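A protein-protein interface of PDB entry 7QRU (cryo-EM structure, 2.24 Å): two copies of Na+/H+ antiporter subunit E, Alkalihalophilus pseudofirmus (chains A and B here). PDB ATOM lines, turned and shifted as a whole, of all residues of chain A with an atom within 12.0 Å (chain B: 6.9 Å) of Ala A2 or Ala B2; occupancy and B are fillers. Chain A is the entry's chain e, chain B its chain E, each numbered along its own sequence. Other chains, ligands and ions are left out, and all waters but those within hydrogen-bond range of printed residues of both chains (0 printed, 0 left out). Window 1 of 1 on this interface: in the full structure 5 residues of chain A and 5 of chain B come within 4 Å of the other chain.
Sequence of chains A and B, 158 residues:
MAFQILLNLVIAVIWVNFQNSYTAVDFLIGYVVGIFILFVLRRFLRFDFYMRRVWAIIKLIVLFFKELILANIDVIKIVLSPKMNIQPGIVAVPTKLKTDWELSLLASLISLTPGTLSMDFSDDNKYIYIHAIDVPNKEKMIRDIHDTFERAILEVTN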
ATOM      1  N   MET A   1     -14.091   0.594  -1.385  1.00  0.00           N
ATOM      2  CA  MET A   1     -13.494   1.905  -1.733  1.00  0.00           C
ATOM      3  C   MET A   1     -12.009   1.749  -2.071  1.00  0.00           C
ATOM      4  O   MET A   1     -11.483   2.507  -2.931  1.00  0.00           O
ATOM      5  CB  MET A   1     -13.628   2.938  -0.597  1.00  0.00           C
ATOM      6  CG  MET A   1     -12.642   4.165  -0.779  1.00  0.00           C
ATOM      7  SD  MET A   1     -12.861   5.584   0.345  1.00  0.00           S
ATOM      8  CE  MET A   1     -11.521   6.685  -0.106  1.00  0.00           C
ATOM      9  N   ALA A   2     -11.295   0.858  -1.357  1.00  0.00           N
ATOM     10  CA  ALA A   2      -9.909   0.617  -1.729  1.00  0.00           C
ATOM     11  C   ALA A   2      -9.914  -0.088  -3.082  1.00  0.00           C
ATOM     12  O   ALA A   2      -9.187   0.341  -3.990  1.00  0.00           O
ATOM     13  CB  ALA A   2      -9.218  -0.208  -0.694  1.00  0.00           C
ATOM     14  N   PHE A   3     -10.818  -1.093  -3.239  1.00  0.00           N
ATOM     15  CA  PHE A   3     -11.051  -1.687  -4.555  1.00  0.00           C
ATOM     16  C   PHE A   3     -11.237  -0.657  -5.674  1.00  0.00           C
ATOM     17  O   PHE A   3     -10.596  -0.785  -6.735  1.00  0.00           O
ATOM     18  CB  PHE A   3     -12.301  -2.550  -4.647  1.00  0.00           C
ATOM     19  CG  PHE A   3     -12.312  -3.237  -5.997  1.00  0.00           C
ATOM     20  CD1 PHE A   3     -11.185  -3.935  -6.449  1.00  0.00           C
ATOM     21  CD2 PHE A   3     -13.367  -3.048  -6.879  1.00  0.00           C
ATOM     22  CE1 PHE A   3     -11.143  -4.473  -7.727  1.00  0.00           C
ATOM     23  CE2 PHE A   3     -13.329  -3.618  -8.141  1.00  0.00           C
ATOM     24  CZ  PHE A   3     -12.218  -4.316  -8.563  1.00  0.00           C
ATOM     25  N   GLN A   4     -12.172   0.306  -5.491  1.00  0.00           N
ATOM     26  CA  GLN A   4     -12.446   1.252  -6.556  1.00  0.00           C
ATOM     27  C   GLN A   4     -11.254   2.142  -6.806  1.00  0.00           C
ATOM     28  O   GLN A   4     -11.023   2.567  -7.967  1.00  0.00           O
ATOM     29  CB  GLN A   4     -13.705   2.041  -6.283  1.00  0.00           C
ATOM     30  CG  GLN A   4     -14.901   1.162  -5.881  1.00  0.00           C
ATOM     31  CD  GLN A   4     -16.095   2.048  -5.648  1.00  0.00           C
ATOM     32  OE1 GLN A   4     -16.193   3.053  -6.346  1.00  0.00           O
ATOM     33  NE2 GLN A   4     -17.003   1.695  -4.716  1.00  0.00           N
ATOM     34  N   ILE A   5     -10.459   2.436  -5.779  1.00  0.00           N
ATOM     35  CA  ILE A   5      -9.343   3.354  -6.042  1.00  0.00           C
ATOM     36  C   ILE A   5      -8.290   2.661  -6.892  1.00  0.00           C
ATOM     37  O   ILE A   5      -7.578   3.329  -7.661  1.00  0.00           O
ATOM     38  CB  ILE A   5      -8.732   3.910  -4.736  1.00  0.00           C
ATOM     39  CG1 ILE A   5      -9.781   4.693  -3.964  1.00  0.00           C
ATOM     40  CG2 ILE A   5      -7.531   4.770  -5.023  1.00  0.00           C
ATOM     41  CD1 ILE A   5      -9.278   5.376  -2.792  1.00  0.00           C
ATOM     42  N   LEU A   6      -8.092   1.356  -6.611  1.00  0.00           N
ATOM     43  CA  LEU A   6      -7.102   0.565  -7.331  1.00  0.00           C
ATOM     44  C   LEU A   6      -7.579   0.305  -8.755  1.00  0.00           C
ATOM     45  O   LEU A   6      -6.747   0.403  -9.672  1.00  0.00           O
ATOM     46  CB  LEU A   6      -6.906  -0.759  -6.588  1.00  0.00           C
ATOM     47  CG  LEU A   6      -5.795  -1.643  -7.120  1.00  0.00           C
ATOM     48  CD1 LEU A   6      -4.477  -0.889  -7.020  1.00  0.00           C
ATOM     49  CD2 LEU A   6      -5.797  -2.976  -6.372  1.00  0.00           C
ATOM     50  N   LEU A   7      -8.885  -0.072  -8.924  1.00  0.00           N
ATOM     51  CA  LEU A   7      -9.491  -0.098 -10.266  1.00  0.00           C
ATOM     52  C   LEU A   7      -9.138   1.193 -11.003  1.00  0.00           C
ATOM     53  O   LEU A   7      -8.857   1.191 -12.167  1.00  0.00           O
ATOM     54  CB  LEU A   7     -10.996  -0.278 -10.198  1.00  0.00           C
ATOM     55  CG  LEU A   7     -11.513  -1.612 -10.649  1.00  0.00           C
ATOM     56  CD1 LEU A   7     -12.980  -1.509 -10.907  1.00  0.00           C
ATOM     57  CD2 LEU A   7     -10.771  -1.985 -11.924  1.00  0.00           C
ATOM     58  N   ASN A   8      -9.335   2.327 -10.389  1.00  0.00           N
ATOM     59  CA  ASN A   8      -9.104   3.572 -11.059  1.00  0.00           C
ATOM     60  C   ASN A   8      -7.647   3.639 -11.454  1.00  0.00           C
ATOM     61  O   ASN A   8      -7.307   4.190 -12.482  1.00  0.00           O
ATOM     62  CB  ASN A   8      -9.473   4.711 -10.105  1.00  0.00           C
ATOM     63  CG  ASN A   8     -10.195   5.865 -10.711  1.00  0.00           C
ATOM     64  OD1 ASN A   8      -9.923   6.270 -11.824  1.00  0.00           O
ATOM     65  ND2 ASN A   8     -11.094   6.432  -9.901  1.00  0.00           N
ATOM     66  N   LEU A   9      -6.711   3.219 -10.570  1.00  0.00           N
ATOM     67  CA  LEU A   9      -5.285   3.190 -10.915  1.00  0.00           C
ATOM     68  C   LEU A   9      -4.987   2.124 -11.977  1.00  0.00           C
ATOM     69  O   LEU A   9      -4.204   2.392 -12.882  1.00  0.00           O
ATOM     70  CB  LEU A   9      -4.496   2.866  -9.644  1.00  0.00           C
ATOM     71  CG  LEU A   9      -4.366   3.985  -8.628  1.00  0.00           C
ATOM     72  CD1 LEU A   9      -3.881   3.357  -7.372  1.00  0.00           C
ATOM     73  CD2 LEU A   9      -3.436   5.089  -9.125  1.00  0.00           C
ATOM     74  N   VAL A  10      -5.627   0.923 -11.869  1.00  0.00           N
ATOM     75  CA  VAL A  10      -5.600  -0.058 -12.973  1.00  0.00           C
ATOM     76  C   VAL A  10      -6.094   0.525 -14.335  1.00  0.00           C
ATOM     77  O   VAL A  10      -5.461   0.306 -15.356  1.00  0.00           O
ATOM     78  CB  VAL A  10      -6.420  -1.308 -12.677  1.00  0.00           C
ATOM     79  CG1 VAL A  10      -6.568  -2.102 -13.973  1.00  0.00           C
ATOM     80  CG2 VAL A  10      -5.863  -2.201 -11.588  1.00  0.00           C
ATOM     81  N   ILE A  11      -7.184   1.334 -14.380  1.00  0.00           N
ATOM     82  CA  ILE A  11      -7.576   2.033 -15.569  1.00  0.00           C
ATOM     83  C   ILE A  11      -6.446   2.950 -16.020  1.00  0.00           C
ATOM     84  O   ILE A  11      -6.170   3.115 -17.236  1.00  0.00           O
ATOM     85  CB  ILE A  11      -8.889   2.822 -15.472  1.00  0.00           C
ATOM     86  CG1 ILE A  11     -10.134   1.966 -15.307  1.00  0.00           C
ATOM     87  CG2 ILE A  11      -9.014   3.791 -16.684  1.00  0.00           C
ATOM     88  CD1 ILE A  11     -10.320   1.025 -16.435  1.00  0.00           C
ATOM     89  N   TYR A  31      -6.435   9.250 -14.787  1.00  0.00           N
ATOM     90  CA  TYR A  31      -6.961   8.839 -13.477  1.00  0.00           C
ATOM     91  C   TYR A  31      -8.409   9.301 -13.470  1.00  0.00           C
ATOM     92  O   TYR A  31      -9.273   8.564 -12.954  1.00  0.00           O
ATOM     93  CB  TYR A  31      -6.158   9.387 -12.280  1.00  0.00           C
ATOM     94  CG  TYR A  31      -6.713   8.868 -10.986  1.00  0.00           C
ATOM     95  CD1 TYR A  31      -6.306   7.646 -10.509  1.00  0.00           C
ATOM     96  CD2 TYR A  31      -7.766   9.531 -10.355  1.00  0.00           C
ATOM     97  CE1 TYR A  31      -6.917   7.059  -9.424  1.00  0.00           C
ATOM     98  CE2 TYR A  31      -8.382   8.964  -9.263  1.00  0.00           C
ATOM     99  CZ  TYR A  31      -7.940   7.741  -8.796  1.00  0.00           C
ATOM    100  OH  TYR A  31      -8.590   7.166  -7.741  1.00  0.00           O
ATOM    101  N   GLY A  34     -10.822   7.088 -15.539  1.00  0.00           N
ATOM    102  CA  GLY A  34     -11.339   5.967 -14.778  1.00  0.00           C
ATOM    103  C   GLY A  34     -12.418   6.379 -13.820  1.00  0.00           C
ATOM    104  O   GLY A  34     -13.286   5.562 -13.593  1.00  0.00           O
ATOM    105  N   ILE A  35     -12.380   7.626 -13.261  1.00  0.00           N
ATOM    106  CA  ILE A  35     -13.449   8.083 -12.340  1.00  0.00           C
ATOM    107  C   ILE A  35     -14.775   8.121 -13.084  1.00  0.00           C
ATOM    108  O   ILE A  35     -15.746   7.599 -12.610  1.00  0.00           O
ATOM    109  CB  ILE A  35     -13.129   9.484 -11.751  1.00  0.00           C
ATOM    110  CG1 ILE A  35     -11.876   9.423 -10.884  1.00  0.00           C
ATOM    111  CG2 ILE A  35     -14.193  10.111 -10.984  1.00  0.00           C
ATOM    112  CD1 ILE A  35     -11.473  10.809 -10.504  1.00  0.00           C
ATOM    113  N   LEU A  38     -16.065   4.606 -13.769  1.00  0.00           N
ATOM    114  CA  LEU A  38     -16.579   3.984 -12.562  1.00  0.00           C
ATOM    115  C   LEU A  38     -17.927   4.572 -12.187  1.00  0.00           C
ATOM    116  O   LEU A  38     -18.843   3.887 -11.779  1.00  0.00           O
ATOM    117  CB  LEU A  38     -15.552   4.196 -11.455  1.00  0.00           C
ATOM    118  CG  LEU A  38     -14.355   3.233 -11.466  1.00  0.00           C
ATOM    119  CD1 LEU A  38     -13.273   3.625 -10.473  1.00  0.00           C
ATOM    120  CD2 LEU A  38     -14.815   1.908 -11.100  1.00  0.00           C
ATOM    121  N   ARG A  46     -22.668  -2.301  -9.051  1.00  0.00           N
ATOM    122  CA  ARG A  46     -23.121  -2.092  -7.675  1.00  0.00           C
ATOM    123  C   ARG A  46     -22.139  -1.316  -6.745  1.00  0.00           C
ATOM    124  O   ARG A  46     -22.276  -1.300  -5.524  1.00  0.00           O
ATOM    125  CB  ARG A  46     -23.388  -3.464  -7.086  1.00  0.00           C
ATOM    126  CG  ARG A  46     -24.353  -4.337  -7.876  1.00  0.00           C
ATOM    127  CD  ARG A  46     -25.802  -3.887  -7.838  1.00  0.00           C
ATOM    128  NE  ARG A  46     -26.190  -3.499  -6.487  1.00  0.00           N
ATOM    129  CZ  ARG A  46     -26.517  -4.345  -5.507  1.00  0.00           C
ATOM    130  NH1 ARG A  46     -26.582  -5.646  -5.735  1.00  0.00           N
ATOM    131  NH2 ARG A  46     -26.788  -3.883  -4.295  1.00  0.00           N
ATOM    132  N   PHE A  47     -21.147  -0.615  -7.287  1.00  0.00           N
ATOM    133  CA  PHE A  47     -20.270   0.215  -6.480  1.00  0.00           C
ATOM    134  C   PHE A  47     -21.167   1.221  -5.724  1.00  0.00           C
ATOM    135  O   PHE A  47     -20.608   1.885  -4.744  1.00  0.00           O
ATOM    136  CB  PHE A  47     -19.230   0.922  -7.366  1.00  0.00           C
ATOM    137  CG  PHE A  47     -18.269  -0.023  -8.013  1.00  0.00           C
ATOM    138  CD1 PHE A  47     -17.908  -1.185  -7.342  1.00  0.00           C
ATOM    139  CD2 PHE A  47     -17.586   0.321  -9.172  1.00  0.00           C
ATOM    140  CE1 PHE A  47     -16.943  -2.038  -7.839  1.00  0.00           C
ATOM    141  CE2 PHE A  47     -16.648  -0.573  -9.679  1.00  0.00           C
ATOM    142  CZ  PHE A  47     -16.285  -1.715  -8.986  1.00  0.00           C
ATOM    143  N   MET B   1      -6.527  -6.887   0.557  1.00  0.00           N
ATOM    144  CA  MET B   1      -5.529  -6.921  -0.553  1.00  0.00           C
ATOM    145  C   MET B   1      -5.531  -5.549  -1.214  1.00  0.00           C
ATOM    146  O   MET B   1      -4.474  -5.008  -1.527  1.00  0.00           O
ATOM    147  CB  MET B   1      -5.748  -7.997  -1.643  1.00  0.00           C
ATOM    148  CG  MET B   1      -4.532  -8.111  -2.552  1.00  0.00           C
ATOM    149  SD  MET B   1      -4.323  -9.379  -3.840  1.00  0.00           S
ATOM    150  CE  MET B   1      -5.068  -8.466  -5.185  1.00  0.00           C
ATOM    151  N   ALA B   2      -6.722  -4.992  -1.418  1.00  0.00           N
ATOM    152  CA  ALA B   2      -6.813  -3.677  -2.010  1.00  0.00           C
ATOM    153  C   ALA B   2      -6.376  -2.664  -0.968  1.00  0.00           C
ATOM    154  O   ALA B   2      -5.631  -1.760  -1.324  1.00  0.00           O
ATOM    155  CB  ALA B   2      -8.209  -3.433  -2.489  1.00  0.00           C
ATOM    156  N   PHE B   3      -6.804  -2.842   0.304  1.00  0.00           N
ATOM    157  CA  PHE B   3      -6.280  -1.977   1.371  1.00  0.00           C
ATOM    158  C   PHE B   3      -4.736  -1.926   1.359  1.00  0.00           C
ATOM    159  O   PHE B   3      -4.139  -0.854   1.324  1.00  0.00           O
ATOM    160  CB  PHE B   3      -6.767  -2.429   2.742  1.00  0.00           C
ATOM    161  CG  PHE B   3      -6.470  -1.448   3.857  1.00  0.00           C
ATOM    162  CD1 PHE B   3      -6.646  -0.082   3.662  1.00  0.00           C
ATOM    163  CD2 PHE B   3      -6.009  -1.889   5.094  1.00  0.00           C
ATOM    164  CE1 PHE B   3      -6.348   0.820   4.661  1.00  0.00           C
ATOM    165  CE2 PHE B   3      -5.769  -0.980   6.108  1.00  0.00           C
ATOM    166  CZ  PHE B   3      -5.942   0.366   5.887  1.00  0.00           C
ATOM    167  N   GLN B   4      -4.069  -3.084   1.404  1.00  0.00           N
ATOM    168  CA  GLN B   4      -2.625  -3.125   1.523  1.00  0.00           C
ATOM    169  C   GLN B   4      -1.955  -2.538   0.289  1.00  0.00           C
ATOM    170  O   GLN B   4      -0.956  -1.830   0.436  1.00  0.00           O
ATOM    171  CB  GLN B   4      -2.162  -4.547   1.828  1.00  0.00           C
ATOM    172  CG  GLN B   4      -2.825  -5.092   3.097  1.00  0.00           C
ATOM    173  CD  GLN B   4      -2.576  -6.566   3.259  1.00  0.00           C
ATOM    174  OE1 GLN B   4      -1.456  -7.025   3.111  1.00  0.00           O
ATOM    175  NE2 GLN B   4      -3.600  -7.304   3.637  1.00  0.00           N
ATOM    176  N   ILE B   5      -2.464  -2.807  -0.917  1.00  0.00           N
ATOM    177  CA  ILE B   5      -1.807  -2.276  -2.109  1.00  0.00           C
ATOM    178  C   ILE B   5      -1.854  -0.750  -2.071  1.00  0.00           C
ATOM    179  O   ILE B   5      -0.874  -0.065  -2.376  1.00  0.00           O
ATOM    180  CB  ILE B   5      -2.430  -2.819  -3.420  1.00  0.00           C
ATOM    181  CG1 ILE B   5      -2.270  -4.327  -3.527  1.00  0.00           C
ATOM    182  CG2 ILE B   5      -1.828  -2.110  -4.625  1.00  0.00           C
ATOM    183  CD1 ILE B   5      -2.895  -4.935  -4.714  1.00  0.00           C
ATOM    184  N   LEU B   6      -3.018  -0.226  -1.690  1.00  0.00           N
ATOM    185  CA  LEU B   6      -3.193   1.216  -1.602  1.00  0.00           C
ATOM    186  C   LEU B   6      -2.222   1.807  -0.576  1.00  0.00           C
ATOM    187  O   LEU B   6      -1.604   2.832  -0.874  1.00  0.00           O
ATOM    188  CB  LEU B   6      -4.651   1.524  -1.220  1.00  0.00           C
ATOM    189  CG  LEU B   6      -5.004   2.995  -1.358  1.00  0.00           C
ATOM    190  CD1 LEU B   6      -4.711   3.411  -2.798  1.00  0.00           C
ATOM    191  CD2 LEU B   6      -6.444   3.279  -0.918  1.00  0.00           C
ATOM    192  N   LEU B   7      -2.150   1.200   0.640  1.00  0.00           N
ATOM    193  CA  LEU B   7      -1.206   1.603   1.682  1.00  0.00           C
ATOM    194  C   LEU B   7       0.206   1.632   1.124  1.00  0.00           C
ATOM    195  O   LEU B   7       0.976   2.534   1.418  1.00  0.00           O
ATOM    196  CB  LEU B   7      -1.185   0.624   2.851  1.00  0.00           C
ATOM    197  CG  LEU B   7      -2.375   0.746   3.773  1.00  0.00           C
ATOM    198  CD1 LEU B   7      -2.294  -0.242   4.907  1.00  0.00           C
ATOM    199  CD2 LEU B   7      -2.468   2.151   4.318  1.00  0.00           C
ATOM    200  N   ASN B   8       0.566   0.595   0.400  1.00  0.00           N
ATOM    201  CA  ASN B   8       1.914   0.466  -0.092  1.00  0.00           C
ATOM    202  C   ASN B   8       2.228   1.611  -1.035  1.00  0.00           C
ATOM    203  O   ASN B   8       3.330   2.161  -1.009  1.00  0.00           O
ATOM    204  CB  ASN B   8       2.103  -0.902  -0.731  1.00  0.00           C
ATOM    205  CG  ASN B   8       3.534  -1.376  -0.692  1.00  0.00           C
ATOM    206  OD1 ASN B   8       4.463  -0.606  -0.974  1.00  0.00           O
ATOM    207  ND2 ASN B   8       3.691  -2.642  -0.336  1.00  0.00           N
ATOM    208  N   TYR B  50      -0.415  -9.271   1.517  1.00  0.00           N
ATOM    209  CA  TYR B  50      -1.047  -9.316   0.192  1.00  0.00           C
ATOM    210  C   TYR B  50      -0.146 -10.039  -0.796  1.00  0.00           C
ATOM    211  O   TYR B  50      -0.666 -10.550  -1.778  1.00  0.00           O
ATOM    212  CB  TYR B  50      -1.440  -7.923  -0.357  1.00  0.00           C
ATOM    213  CG  TYR B  50      -0.315  -7.038  -0.827  1.00  0.00           C
ATOM    214  CD1 TYR B  50       0.585  -6.464   0.061  1.00  0.00           C
ATOM    215  CD2 TYR B  50      -0.140  -6.780  -2.154  1.00  0.00           C
ATOM    216  CE1 TYR B  50       1.586  -5.606  -0.352  1.00  0.00           C
ATOM    217  CE2 TYR B  50       0.854  -5.915  -2.601  1.00  0.00           C
ATOM    218  CZ  TYR B  50       1.723  -5.332  -1.703  1.00  0.00           C
ATOM    219  OH  TYR B  50       2.768  -4.573  -2.145  1.00  0.00           O
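Among the printed residues, no Asp or Glu carboxylate lies within 4 Å of a Lys or Arg side-chain nitrogen of the other chain.
Ala A2 touches its own counterpart, Ala B2. Ala A2 touches Phe B3, and with the chains exchanged Phe A3 touches Ala B2. Ile A5 touches Leu B6, and with the chains exchanged Leu A6 touches Ile B5. 8 positions are printed for both chains.
Among the printed residues, merely in contact across the chains: Phe A3 with Ala B2 (3.6 Å), Ala A2 with Phe B3 (3.7 Å), Ala A2 with Ala B2 (3.8 Å), Leu A6 with Ile B5 (3.8 Å) and Ile A5 with Leu B6 (3.8 Å).
Ala A2 touches just these residues of chain B: Ala B2 (3.8 Å) and Phe B3 (3.7 Å). Printed residues of chain B within 4 Å of Phe A3: Ala B2. Of the printed residues of chain B, Ile A5 touches Leu B6. Of the printed residues of chain B, Leu A6 touches Ile B5 (3.8 Å). Of chain A, only Ala A2 (3.8 Å) and Phe A3 (3.6 Å) come within 4 Å of Ala B2. No residue of chain A comes within 4 Å of Gln B4. Leu B6 touches just one residue of chain A: Ile A5 (3.8 Å). The nearest residue of chain B that does not touch Ala A2 is Leu B6 (4.4 Å). The nearest residue of chain A that does not touch Ala B2 is Leu A6 (4.5 Å). The nearest printed residue of chain B that does not touch Leu A6 is Ala B2 (4.5 Å).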
